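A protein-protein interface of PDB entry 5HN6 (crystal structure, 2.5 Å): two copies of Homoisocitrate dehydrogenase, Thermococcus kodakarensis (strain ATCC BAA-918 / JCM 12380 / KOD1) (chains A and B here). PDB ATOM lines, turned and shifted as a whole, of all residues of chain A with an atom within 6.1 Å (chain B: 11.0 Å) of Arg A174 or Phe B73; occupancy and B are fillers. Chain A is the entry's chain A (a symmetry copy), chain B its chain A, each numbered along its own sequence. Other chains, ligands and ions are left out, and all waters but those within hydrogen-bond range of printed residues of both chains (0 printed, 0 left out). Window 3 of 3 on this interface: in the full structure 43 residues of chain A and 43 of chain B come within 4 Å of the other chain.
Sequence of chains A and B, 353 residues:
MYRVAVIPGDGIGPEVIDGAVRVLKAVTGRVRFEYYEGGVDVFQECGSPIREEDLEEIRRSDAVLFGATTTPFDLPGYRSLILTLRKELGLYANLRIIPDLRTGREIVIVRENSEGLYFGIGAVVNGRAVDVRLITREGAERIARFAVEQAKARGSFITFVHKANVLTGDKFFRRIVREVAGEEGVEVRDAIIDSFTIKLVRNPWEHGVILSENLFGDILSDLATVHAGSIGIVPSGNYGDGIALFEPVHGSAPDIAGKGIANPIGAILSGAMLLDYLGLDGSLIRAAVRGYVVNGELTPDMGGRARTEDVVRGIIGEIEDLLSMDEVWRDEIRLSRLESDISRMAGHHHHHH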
ATOM      1  N   PHE A 160     -22.210   3.608  35.185  1.00  0.00           N
ATOM      2  CA  PHE A 160     -22.206   2.489  34.276  1.00  0.00           C
ATOM      3  C   PHE A 160     -21.008   1.567  34.546  1.00  0.00           C
ATOM      4  O   PHE A 160     -19.867   1.935  34.281  1.00  0.00           O
ATOM      5  CB  PHE A 160     -22.266   2.919  32.801  1.00  0.00           C
ATOM      6  CG  PHE A 160     -22.312   1.756  31.856  1.00  0.00           C
ATOM      7  CD1 PHE A 160     -23.356   0.826  31.928  1.00  0.00           C
ATOM      8  CD2 PHE A 160     -21.281   1.527  30.957  1.00  0.00           C
ATOM      9  CE1 PHE A 160     -23.373  -0.289  31.088  1.00  0.00           C
ATOM     10  CE2 PHE A 160     -21.278   0.414  30.137  1.00  0.00           C
ATOM     11  CZ  PHE A 160     -22.324  -0.509  30.212  1.00  0.00           C
ATOM     12  N   HIS A 162     -18.770  -1.817  33.904  1.00  0.00           N
ATOM     13  CA  HIS A 162     -18.433  -2.561  32.704  1.00  0.00           C
ATOM     14  C   HIS A 162     -17.004  -3.031  32.747  1.00  0.00           C
ATOM     15  O   HIS A 162     -16.312  -2.790  33.728  1.00  0.00           O
ATOM     16  CB  HIS A 162     -18.610  -1.692  31.495  1.00  0.00           C
ATOM     17  CG  HIS A 162     -17.663  -0.549  31.429  1.00  0.00           C
ATOM     18  ND1 HIS A 162     -17.977   0.708  31.905  1.00  0.00           N
ATOM     19  CD2 HIS A 162     -16.418  -0.454  30.925  1.00  0.00           C
ATOM     20  CE1 HIS A 162     -16.959   1.522  31.702  1.00  0.00           C
ATOM     21  NE2 HIS A 162     -16.000   0.843  31.107  1.00  0.00           N
ATOM     22  N   ALA A 164     -15.137  -2.744  29.510  1.00  0.00           N
ATOM     23  CA  ALA A 164     -15.051  -2.354  28.125  1.00  0.00           C
ATOM     24  C   ALA A 164     -13.599  -2.376  27.663  1.00  0.00           C
ATOM     25  O   ALA A 164     -13.338  -2.411  26.467  1.00  0.00           O
ATOM     26  CB  ALA A 164     -15.683  -0.986  27.917  1.00  0.00           C
ATOM     27  N   ASN A 165     -12.669  -2.445  28.615  1.00  0.00           N
ATOM     28  CA  ASN A 165     -11.243  -2.710  28.320  1.00  0.00           C
ATOM     29  C   ASN A 165     -10.971  -4.109  27.757  1.00  0.00           C
ATOM     30  O   ASN A 165      -9.922  -4.369  27.180  1.00  0.00           O
ATOM     31  CB  ASN A 165     -10.327  -2.390  29.543  1.00  0.00           C
ATOM     32  CG  ASN A 165     -10.894  -2.907  30.896  1.00  0.00           C
ATOM     33  OD1 ASN A 165     -12.084  -3.235  31.003  1.00  0.00           O
ATOM     34  ND2 ASN A 165     -10.031  -2.983  31.936  1.00  0.00           N
ATOM     35  N   GLY A 169     -18.678  -6.046  23.485  1.00  0.00           N
ATOM     36  CA  GLY A 169     -20.034  -5.691  23.819  1.00  0.00           C
ATOM     37  C   GLY A 169     -20.164  -4.630  24.876  1.00  0.00           C
ATOM     38  O   GLY A 169     -21.153  -3.885  24.896  1.00  0.00           O
ATOM     39  N   ASP A 170     -19.214  -4.540  25.799  1.00  0.00           N
ATOM     40  CA  ASP A 170     -19.300  -3.448  26.799  1.00  0.00           C
ATOM     41  C   ASP A 170     -18.874  -2.104  26.215  1.00  0.00           C
ATOM     42  O   ASP A 170     -19.415  -1.081  26.604  1.00  0.00           O
ATOM     43  CB  ASP A 170     -18.508  -3.768  28.048  1.00  0.00           C
ATOM     44  CG  ASP A 170     -19.361  -4.349  29.161  1.00  0.00           C
ATOM     45  OD1 ASP A 170     -20.620  -4.418  29.050  1.00  0.00           O
ATOM     46  OD2 ASP A 170     -18.752  -4.685  30.197  1.00  0.00           O
ATOM     47  N   LYS A 171     -17.918  -2.098  25.286  1.00  0.00           N
ATOM     48  CA  LYS A 171     -17.619  -0.886  24.494  1.00  0.00           C
ATOM     49  C   LYS A 171     -18.884  -0.363  23.804  1.00  0.00           C
ATOM     50  O   LYS A 171     -19.239   0.801  23.958  1.00  0.00           O
ATOM     51  CB  LYS A 171     -16.537  -1.138  23.432  1.00  0.00           C
ATOM     52  CG  LYS A 171     -15.125  -1.206  23.984  1.00  0.00           C
ATOM     53  CD  LYS A 171     -14.056  -1.227  22.890  1.00  0.00           C
ATOM     54  CE  LYS A 171     -13.852   0.145  22.244  1.00  0.00           C
ATOM     55  NZ  LYS A 171     -13.527   1.205  23.239  1.00  0.00           N
ATOM     56  N   PHE A 172     -19.550  -1.241  23.052  1.00  0.00           N
ATOM     57  CA  PHE A 172     -20.810  -0.923  22.386  1.00  0.00           C
ATOM     58  C   PHE A 172     -21.843  -0.413  23.378  1.00  0.00           C
ATOM     59  O   PHE A 172     -22.417   0.654  23.192  1.00  0.00           O
ATOM     60  CB  PHE A 172     -21.307  -2.164  21.681  1.00  0.00           C
ATOM     61  CG  PHE A 172     -22.579  -1.974  20.932  1.00  0.00           C
ATOM     62  CD1 PHE A 172     -22.578  -1.341  19.697  1.00  0.00           C
ATOM     63  CD2 PHE A 172     -23.764  -2.461  21.434  1.00  0.00           C
ATOM     64  CE1 PHE A 172     -23.740  -1.180  18.994  1.00  0.00           C
ATOM     65  CE2 PHE A 172     -24.930  -2.306  20.735  1.00  0.00           C
ATOM     66  CZ  PHE A 172     -24.919  -1.658  19.517  1.00  0.00           C
ATOM     67  N   PHE A 173     -22.044  -1.164  24.457  1.00  0.00           N
ATOM     68  CA  PHE A 173     -23.042  -0.821  25.457  1.00  0.00           C
ATOM     69  C   PHE A 173     -22.791   0.588  25.981  1.00  0.00           C
ATOM     70  O   PHE A 173     -23.724   1.335  26.270  1.00  0.00           O
ATOM     71  CB  PHE A 173     -22.958  -1.841  26.610  1.00  0.00           C
ATOM     72  CG  PHE A 173     -24.169  -1.914  27.505  1.00  0.00           C
ATOM     73  CD1 PHE A 173     -25.203  -0.990  27.461  1.00  0.00           C
ATOM     74  CD2 PHE A 173     -24.241  -2.932  28.454  1.00  0.00           C
ATOM     75  CE1 PHE A 173     -26.287  -1.096  28.325  1.00  0.00           C
ATOM     76  CE2 PHE A 173     -25.297  -3.023  29.332  1.00  0.00           C
ATOM     77  CZ  PHE A 173     -26.331  -2.115  29.258  1.00  0.00           C
ATOM     78  N   ARG A 174     -21.521   0.931  26.125  1.00  0.00           N
ATOM     79  CA  ARG A 174     -21.112   2.194  26.731  1.00  0.00           C
ATOM     80  C   ARG A 174     -21.477   3.365  25.832  1.00  0.00           C
ATOM     81  O   ARG A 174     -22.090   4.312  26.302  1.00  0.00           O
ATOM     82  CB  ARG A 174     -19.613   2.201  27.036  1.00  0.00           C
ATOM     83  CG  ARG A 174     -19.172   3.355  27.945  1.00  0.00           C
ATOM     84  CD  ARG A 174     -17.658   3.384  28.049  1.00  0.00           C
ATOM     85  NE  ARG A 174     -17.167   4.526  28.808  1.00  0.00           N
ATOM     86  CZ  ARG A 174     -16.621   5.626  28.283  1.00  0.00           C
ATOM     87  NH1 ARG A 174     -16.201   6.601  29.078  1.00  0.00           N
ATOM     88  NH2 ARG A 174     -16.487   5.772  26.978  1.00  0.00           N
ATOM     89  N   ARG A 175     -21.135   3.279  24.549  1.00  0.00           N
ATOM     90  CA  ARG A 175     -21.546   4.289  23.571  1.00  0.00           C
ATOM     91  C   ARG A 175     -22.996   4.596  23.788  1.00  0.00           C
ATOM     92  O   ARG A 175     -23.373   5.766  23.963  1.00  0.00           O
ATOM     93  CB  ARG A 175     -21.394   3.804  22.128  1.00  0.00           C
ATOM     94  CG  ARG A 175     -20.087   4.174  21.451  1.00  0.00           C
ATOM     95  CD  ARG A 175     -20.181   4.131  19.928  1.00  0.00           C
ATOM     96  NE  ARG A 175     -20.939   2.996  19.375  1.00  0.00           N
ATOM     97  CZ  ARG A 175     -22.076   3.085  18.675  1.00  0.00           C
ATOM     98  NH1 ARG A 175     -22.644   4.260  18.410  1.00  0.00           N
ATOM     99  NH2 ARG A 175     -22.661   1.976  18.230  1.00  0.00           N
ATOM    100  N   ILE A 176     -23.813   3.546  23.794  1.00  0.00           N
ATOM    101  CA  ILE A 176     -25.241   3.756  23.740  1.00  0.00           C
ATOM    102  C   ILE A 176     -25.758   4.350  25.030  1.00  0.00           C
ATOM    103  O   ILE A 176     -26.593   5.240  24.995  1.00  0.00           O
ATOM    104  CB  ILE A 176     -26.020   2.499  23.280  1.00  0.00           C
ATOM    105  CG1 ILE A 176     -25.807   2.291  21.795  1.00  0.00           C
ATOM    106  CG2 ILE A 176     -27.513   2.660  23.521  1.00  0.00           C
ATOM    107  CD1 ILE A 176     -25.958   0.871  21.340  1.00  0.00           C
ATOM    108  N   VAL A 177     -25.247   3.922  26.169  1.00  0.00           N
ATOM    109  CA  VAL A 177     -25.687   4.548  27.427  1.00  0.00           C
ATOM    110  C   VAL A 177     -25.289   6.033  27.495  1.00  0.00           C
ATOM    111  O   VAL A 177     -26.023   6.846  28.043  1.00  0.00           O
ATOM    112  CB  VAL A 177     -25.157   3.788  28.653  1.00  0.00           C
ATOM    113  CG1 VAL A 177     -25.441   4.545  29.942  1.00  0.00           C
ATOM    114  CG2 VAL A 177     -25.784   2.407  28.730  1.00  0.00           C
ATOM    115  N   ARG A 178     -24.129   6.381  26.947  1.00  0.00           N
ATOM    116  CA  ARG A 178     -23.659   7.774  26.966  1.00  0.00           C
ATOM    117  C   ARG A 178     -24.509   8.618  26.009  1.00  0.00           C
ATOM    118  O   ARG A 178     -25.017   9.661  26.393  1.00  0.00           O
ATOM    119  CB  ARG A 178     -22.145   7.849  26.682  1.00  0.00           C
ATOM    120  CG  ARG A 178     -21.331   7.192  27.821  1.00  0.00           C
ATOM    121  CD  ARG A 178     -19.841   7.532  27.893  1.00  0.00           C
ATOM    122  NE  ARG A 178     -19.663   8.955  28.192  1.00  0.00           N
ATOM    123  CZ  ARG A 178     -19.096   9.847  27.383  1.00  0.00           C
ATOM    124  NH1 ARG A 178     -18.578   9.490  26.216  1.00  0.00           N
ATOM    125  NH2 ARG A 178     -19.033  11.110  27.762  1.00  0.00           N
ATOM    126  N   GLU A 179     -24.718   8.122  24.798  1.00  0.00           N
ATOM    127  CA  GLU A 179     -25.666   8.723  23.895  1.00  0.00           C
ATOM    128  C   GLU A 179     -27.031   8.991  24.517  1.00  0.00           C
ATOM    129  O   GLU A 179     -27.495  10.139  24.470  1.00  0.00           O
ATOM    130  CB  GLU A 179     -25.819   7.874  22.651  1.00  0.00           C
ATOM    131  CG  GLU A 179     -24.608   7.920  21.720  1.00  0.00           C
ATOM    132  CD  GLU A 179     -24.774   7.029  20.485  1.00  0.00           C
ATOM    133  OE1 GLU A 179     -23.750   6.696  19.849  1.00  0.00           O
ATOM    134  OE2 GLU A 179     -25.925   6.655  20.145  1.00  0.00           O
ATOM    135  N   ASP A 190     -18.165   6.376  34.632  1.00  0.00           N
ATOM    136  CA  ASP A 190     -17.616   5.067  34.404  1.00  0.00           C
ATOM    137  C   ASP A 190     -17.253   4.396  35.719  1.00  0.00           C
ATOM    138  O   ASP A 190     -16.883   5.054  36.679  1.00  0.00           O
ATOM    139  CB  ASP A 190     -16.355   5.185  33.566  1.00  0.00           C
ATOM    140  CG  ASP A 190     -16.654   5.421  32.135  1.00  0.00           C
ATOM    141  OD1 ASP A 190     -16.997   4.466  31.435  1.00  0.00           O
ATOM    142  OD2 ASP A 190     -16.557   6.567  31.677  1.00  0.00           O
ATOM    143  N   ILE A 192     -15.338   0.317  36.524  1.00  0.00           N
ATOM    144  CA  ILE A 192     -14.914  -0.928  35.985  1.00  0.00           C
ATOM    145  C   ILE A 192     -15.365  -1.987  36.960  1.00  0.00           C
ATOM    146  O   ILE A 192     -15.348  -1.774  38.168  1.00  0.00           O
ATOM    147  CB  ILE A 192     -13.403  -0.981  35.800  1.00  0.00           C
ATOM    148  CG1 ILE A 192     -12.907   0.265  35.056  1.00  0.00           C
ATOM    149  CG2 ILE A 192     -13.024  -2.235  35.015  1.00  0.00           C
ATOM    150  CD1 ILE A 192     -13.196   0.301  33.574  1.00  0.00           C
ATOM    151  N   VAL B  40       2.225   2.625  26.257  1.00  0.00           N
ATOM    152  CA  VAL B  40       1.766   3.484  25.149  1.00  0.00           C
ATOM    153  C   VAL B  40       2.957   4.070  24.351  1.00  0.00           C
ATOM    154  O   VAL B  40       3.025   3.928  23.130  1.00  0.00           O
ATOM    155  CB  VAL B  40       0.747   4.540  25.618  1.00  0.00           C
ATOM    156  CG1 VAL B  40      -0.311   3.888  26.483  1.00  0.00           C
ATOM    157  CG2 VAL B  40       1.379   5.650  26.417  1.00  0.00           C
ATOM    158  N   PHE B  43       3.947   1.768  21.905  1.00  0.00           N
ATOM    159  CA  PHE B  43       2.911   1.655  20.875  1.00  0.00           C
ATOM    160  C   PHE B  43       3.063   2.745  19.814  1.00  0.00           C
ATOM    161  O   PHE B  43       2.959   2.472  18.620  1.00  0.00           O
ATOM    162  CB  PHE B  43       1.519   1.750  21.501  1.00  0.00           C
ATOM    163  CG  PHE B  43       0.409   1.802  20.504  1.00  0.00           C
ATOM    164  CD1 PHE B  43       0.162   0.717  19.668  1.00  0.00           C
ATOM    165  CD2 PHE B  43      -0.398   2.930  20.401  1.00  0.00           C
ATOM    166  CE1 PHE B  43      -0.858   0.752  18.740  1.00  0.00           C
ATOM    167  CE2 PHE B  43      -1.429   2.969  19.470  1.00  0.00           C
ATOM    168  CZ  PHE B  43      -1.656   1.876  18.643  1.00  0.00           C
ATOM    169  N   THR B  69       0.937  -0.726  34.137  1.00  0.00           N
ATOM    170  CA  THR B  69       0.877  -0.139  32.821  1.00  0.00           C
ATOM    171  C   THR B  69      -0.417   0.591  32.698  1.00  0.00           C
ATOM    172  O   THR B  69      -1.496   0.065  33.038  1.00  0.00           O
ATOM    173  CB  THR B  69       0.981  -1.238  31.751  1.00  0.00           C
ATOM    174  OG1 THR B  69       0.908  -0.653  30.461  1.00  0.00           O
ATOM    175  CG2 THR B  69      -0.149  -2.279  31.887  1.00  0.00           C
ATOM    176  N   THR B  70      -0.337   1.824  32.236  1.00  0.00           N
ATOM    177  CA  THR B  70      -1.550   2.581  32.013  1.00  0.00           C
ATOM    178  C   THR B  70      -2.149   2.167  30.659  1.00  0.00           C
ATOM    179  O   THR B  70      -1.444   2.126  29.644  1.00  0.00           O
ATOM    180  CB  THR B  70      -1.280   4.082  32.088  1.00  0.00           C
ATOM    181  OG1 THR B  70      -0.723   4.384  33.382  1.00  0.00           O
ATOM    182  CG2 THR B  70      -2.604   4.878  31.887  1.00  0.00           C
ATOM    183  N   THR B  71      -3.425   1.796  30.649  1.00  0.00           N
ATOM    184  CA  THR B  71      -4.086   1.500  29.381  1.00  0.00           C
ATOM    185  C   THR B  71      -5.247   2.458  29.133  1.00  0.00           C
ATOM    186  O   THR B  71      -6.373   2.222  29.601  1.00  0.00           O
ATOM    187  CB  THR B  71      -4.547   0.045  29.279  1.00  0.00           C
ATOM    188  OG1 THR B  71      -3.398  -0.817  29.378  1.00  0.00           O
ATOM    189  CG2 THR B  71      -5.290  -0.184  27.911  1.00  0.00           C
ATOM    190  N   PRO B  72      -4.968   3.539  28.394  1.00  0.00           N
ATOM    191  CA  PRO B  72      -5.941   4.598  28.292  1.00  0.00           C
ATOM    192  C   PRO B  72      -7.110   4.076  27.499  1.00  0.00           C
ATOM    193  O   PRO B  72      -6.928   3.361  26.508  1.00  0.00           O
ATOM    194  CB  PRO B  72      -5.192   5.713  27.545  1.00  0.00           C
ATOM    195  CG  PRO B  72      -4.087   5.029  26.796  1.00  0.00           C
ATOM    196  CD  PRO B  72      -3.917   3.644  27.359  1.00  0.00           C
ATOM    197  N   PHE B  73      -8.302   4.402  27.961  1.00  0.00           N
ATOM    198  CA  PHE B  73      -9.506   3.872  27.359  1.00  0.00           C
ATOM    199  C   PHE B  73      -9.752   4.459  25.960  1.00  0.00           C
ATOM    200  O   PHE B  73     -10.324   3.806  25.088  1.00  0.00           O
ATOM    201  CB  PHE B  73     -10.706   4.163  28.262  1.00  0.00           C
ATOM    202  CG  PHE B  73     -11.922   3.461  27.815  1.00  0.00           C
ATOM    203  CD1 PHE B  73     -12.115   2.136  28.157  1.00  0.00           C
ATOM    204  CD2 PHE B  73     -12.830   4.089  26.965  1.00  0.00           C
ATOM    205  CE1 PHE B  73     -13.222   1.454  27.694  1.00  0.00           C
ATOM    206  CE2 PHE B  73     -13.947   3.418  26.513  1.00  0.00           C
ATOM    207  CZ  PHE B  73     -14.149   2.097  26.877  1.00  0.00           C
ATOM    208  N   ASP B  74      -9.289   5.690  25.768  1.00  0.00           N
ATOM    209  CA  ASP B  74      -9.582   6.500  24.593  1.00  0.00           C
ATOM    210  C   ASP B  74      -8.406   6.557  23.612  1.00  0.00           C
ATOM    211  O   ASP B  74      -8.109   7.603  23.051  1.00  0.00           O
ATOM    212  CB  ASP B  74      -9.929   7.915  25.070  1.00  0.00           C
ATOM    213  CG  ASP B  74      -8.865   8.502  26.038  1.00  0.00           C
ATOM    214  OD1 ASP B  74      -8.222   7.728  26.814  1.00  0.00           O
ATOM    215  OD2 ASP B  74      -8.688   9.749  26.026  1.00  0.00           O
ATOM    216  N   LEU B  75      -7.727   5.434  23.416  1.00  0.00           N
ATOM    217  CA  LEU B  75      -6.620   5.370  22.484  1.00  0.00           C
ATOM    218  C   LEU B  75      -6.883   4.230  21.528  1.00  0.00           C
ATOM    219  O   LEU B  75      -6.696   3.073  21.849  1.00  0.00           O
ATOM    220  CB  LEU B  75      -5.308   5.145  23.214  1.00  0.00           C
ATOM    221  CG  LEU B  75      -4.069   4.906  22.339  1.00  0.00           C
ATOM    222  CD1 LEU B  75      -3.683   6.144  21.535  1.00  0.00           C
ATOM    223  CD2 LEU B  75      -2.917   4.476  23.226  1.00  0.00           C
ATOM    224  N   PRO B  76      -7.346   4.550  20.336  1.00  0.00           N
ATOM    225  CA  PRO B  76      -7.744   3.443  19.473  1.00  0.00           C
ATOM    226  C   PRO B  76      -6.580   2.579  18.980  1.00  0.00           C
ATOM    227  O   PRO B  76      -5.478   3.071  18.773  1.00  0.00           O
ATOM    228  CB  PRO B  76      -8.464   4.147  18.311  1.00  0.00           C
ATOM    229  CG  PRO B  76      -8.046   5.583  18.381  1.00  0.00           C
ATOM    230  CD  PRO B  76      -7.754   5.869  19.818  1.00  0.00           C
ATOM    231  N   GLY B  77      -6.854   1.300  18.784  1.00  0.00           N
ATOM    232  CA  GLY B  77      -5.879   0.324  18.317  1.00  0.00           C
ATOM    233  C   GLY B  77      -5.053  -0.371  19.399  1.00  0.00           C
ATOM    234  O   GLY B  77      -4.313  -1.309  19.111  1.00  0.00           O
ATOM    235  N   TYR B  78      -5.165   0.069  20.645  1.00  0.00           N
ATOM    236  CA  TYR B  78      -4.180  -0.305  21.653  1.00  0.00           C
ATOM    237  C   TYR B  78      -4.572  -1.544  22.412  1.00  0.00           C
ATOM    238  O   TYR B  78      -5.589  -1.548  23.095  1.00  0.00           O
ATOM    239  CB  TYR B  78      -3.977   0.841  22.642  1.00  0.00           C
ATOM    240  CG  TYR B  78      -2.899   0.581  23.662  1.00  0.00           C
ATOM    241  CD1 TYR B  78      -1.553   0.636  23.317  1.00  0.00           C
ATOM    242  CD2 TYR B  78      -3.225   0.296  24.978  1.00  0.00           C
ATOM    243  CE1 TYR B  78      -0.567   0.416  24.267  1.00  0.00           C
ATOM    244  CE2 TYR B  78      -2.265   0.072  25.926  1.00  0.00           C
ATOM    245  CZ  TYR B  78      -0.934   0.134  25.576  1.00  0.00           C
ATOM    246  OH  TYR B  78       0.029  -0.099  26.526  1.00  0.00           O
ATOM    247  N   ARG B  79      -3.745  -2.584  22.311  1.00  0.00           N
ATOM    248  CA  ARG B  79      -3.873  -3.763  23.161  1.00  0.00           C
ATOM    249  C   ARG B  79      -3.122  -3.538  24.510  1.00  0.00           C
ATOM    250  O   ARG B  79      -1.961  -3.101  24.505  1.00  0.00           O
ATOM    251  CB  ARG B  79      -3.342  -4.998  22.417  1.00  0.00           C
ATOM    252  CG  ARG B  79      -3.829  -6.329  23.020  1.00  0.00           C
ATOM    253  CD  ARG B  79      -5.174  -6.790  22.444  1.00  0.00           C
ATOM    254  NE  ARG B  79      -5.999  -7.544  23.399  1.00  0.00           N
ATOM    255  CZ  ARG B  79      -6.073  -8.876  23.501  1.00  0.00           C
ATOM    256  NH1 ARG B  79      -6.879  -9.405  24.417  1.00  0.00           N
ATOM    257  NH2 ARG B  79      -5.368  -9.692  22.713  1.00  0.00           N
ATOM    258  N   SER B  80      -3.799  -3.793  25.640  1.00  0.00           N
ATOM    259  CA  SER B  80      -3.147  -3.852  26.974  1.00  0.00           C
ATOM    260  C   SER B  80      -1.830  -4.671  26.961  1.00  0.00           C
ATOM    261  O   SER B  80      -1.799  -5.803  26.502  1.00  0.00           O
ATOM    262  CB  SER B  80      -4.087  -4.470  28.017  1.00  0.00           C
ATOM    263  OG  SER B  80      -3.917  -3.873  29.300  1.00  0.00           O
ATOM    264  N   VAL B 124     -18.991  -6.559  16.570  1.00  0.00           N
ATOM    265  CA  VAL B 124     -20.201  -5.768  16.461  1.00  0.00           C
ATOM    266  C   VAL B 124     -20.619  -5.734  15.009  1.00  0.00           C
ATOM    267  O   VAL B 124     -19.789  -5.552  14.152  1.00  0.00           O
ATOM    268  CB  VAL B 124     -19.992  -4.330  16.887  1.00  0.00           C
ATOM    269  CG1 VAL B 124     -21.353  -3.623  16.981  1.00  0.00           C
ATOM    270  CG2 VAL B 124     -19.233  -4.306  18.198  1.00  0.00           C
ATOM    271  N   ALA B 129     -23.626  -6.659  19.284  1.00  0.00           N
ATOM    272  CA  ALA B 129     -22.251  -6.908  19.714  1.00  0.00           C
ATOM    273  C   ALA B 129     -22.205  -8.130  20.583  1.00  0.00           C
ATOM    274  O   ALA B 129     -23.061  -8.322  21.430  1.00  0.00           O
ATOM    275  CB  ALA B 129     -21.725  -5.720  20.479  1.00  0.00           C
ATOM    276  N   ASP B 131     -19.477 -11.075  22.749  1.00  0.00           N
ATOM    277  CA  ASP B 131     -18.188 -11.568  23.213  1.00  0.00           C
ATOM    278  C   ASP B 131     -18.470 -13.002  23.546  1.00  0.00           C
ATOM    279  O   ASP B 131     -19.545 -13.315  24.104  1.00  0.00           O
ATOM    280  CB  ASP B 131     -17.757 -10.822  24.482  1.00  0.00           C
ATOM    281  CG  ASP B 131     -17.356  -9.405  24.222  1.00  0.00           C
ATOM    282  OD1 ASP B 131     -16.213  -9.182  23.776  1.00  0.00           O
ATOM    283  OD2 ASP B 131     -18.165  -8.505  24.454  1.00  0.00           O
ATOM    284  N   SER B 252      -1.506   1.145  37.717  1.00  0.00           N
ATOM    285  CA  SER B 252      -0.411   2.096  37.529  1.00  0.00           C
ATOM    286  C   SER B 252      -0.620   3.388  38.297  1.00  0.00           C
ATOM    287  O   SER B 252       0.272   4.246  38.294  1.00  0.00           O
ATOM    288  CB  SER B 252      -0.217   2.402  36.041  1.00  0.00           C
ATOM    289  OG  SER B 252      -1.348   3.096  35.563  1.00  0.00           O
ATOM    290  N   PRO B 254      -1.671   6.552  38.210  1.00  0.00           N
ATOM    291  CA  PRO B 254      -0.987   7.776  37.776  1.00  0.00           C
ATOM    292  C   PRO B 254      -1.309   9.000  38.643  1.00  0.00           C
ATOM    293  O   PRO B 254      -0.574   9.970  38.588  1.00  0.00           O
ATOM    294  CB  PRO B 254      -1.465   7.969  36.336  1.00  0.00           C
ATOM    295  CG  PRO B 254      -2.764   7.246  36.259  1.00  0.00           C
ATOM    296  CD  PRO B 254      -2.675   6.103  37.230  1.00  0.00           C
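NH1 of Arg A174 is in salt-bridge range of OD2 of Asp A190.
No position is printed for both chains. Of the 7 pairs that touch across the chains among the printed residues, none has its exchanged pair printed and touching as well.
Ala A164 touches Phe B73 (CB to CE1, 3.5 Å). CA of Gly A169 touches CB of Ala B129 (3.7 Å). Lys A171 touches Phe B73 (NZ to CZ, 3.8 Å). Val B124 touches Phe A172. Phe A172 touches Ala B129. Arg A174 touches Phe B73.
Arg A174 touches one residue of chain B. Of chain A, only Ala A164, Lys A171 and Arg A174 come within 4 Å of Phe B73. No residue of chain B comes within 4 Å of Asn A165. Of chain B, only Phe B73 comes within 4 Å of Lys A171. Ile A176 touches none of the printed residues of chain B. No residue of chain B comes within 4 Å of Val A177. No residue of chain B comes within 4 Å of Arg A178. Of the printed residues of chain B, Phe A172 touches Val B124 and Ala B129. Of the printed residues of chain A, Ala B129 touches Gly A169 (3.7 Å) and Phe A172 (3.8 Å). Printed residues of chain A within 4 Å of Asp B131: Gly A169 (2.7 Å). Ile A192 touches none of the printed residues of chain B. Pro B72 touches none of the printed residues of chain A. The nearest residue of chain B that does not touch Arg A174 is Asp B74 (7.2 Å). The nearest printed residue of chain A that does not touch Ala B129 is Asp A170 (6.0 Å).
The backbone NH (N) of Gly A169 is in hydrogen-bond range of the side-chain carboxylate (OD2) of Asp B131, 2.7 Å away.
Of the 17 printed residues of chain A, 5 touch a printed residue of chain B. Hydrophobic or aromatic side chains of chain A that line the printed part of chain B: Ala A164 and Phe A172. Hydrophobic or aromatic side chains of chain B that line the printed part of chain A: Phe B73, Val B124 and Ala B129. Among the printed residues, no Asp or Glu carboxylate lies within 4 Å of a Lys or Arg side-chain nitrogen of the other chain.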
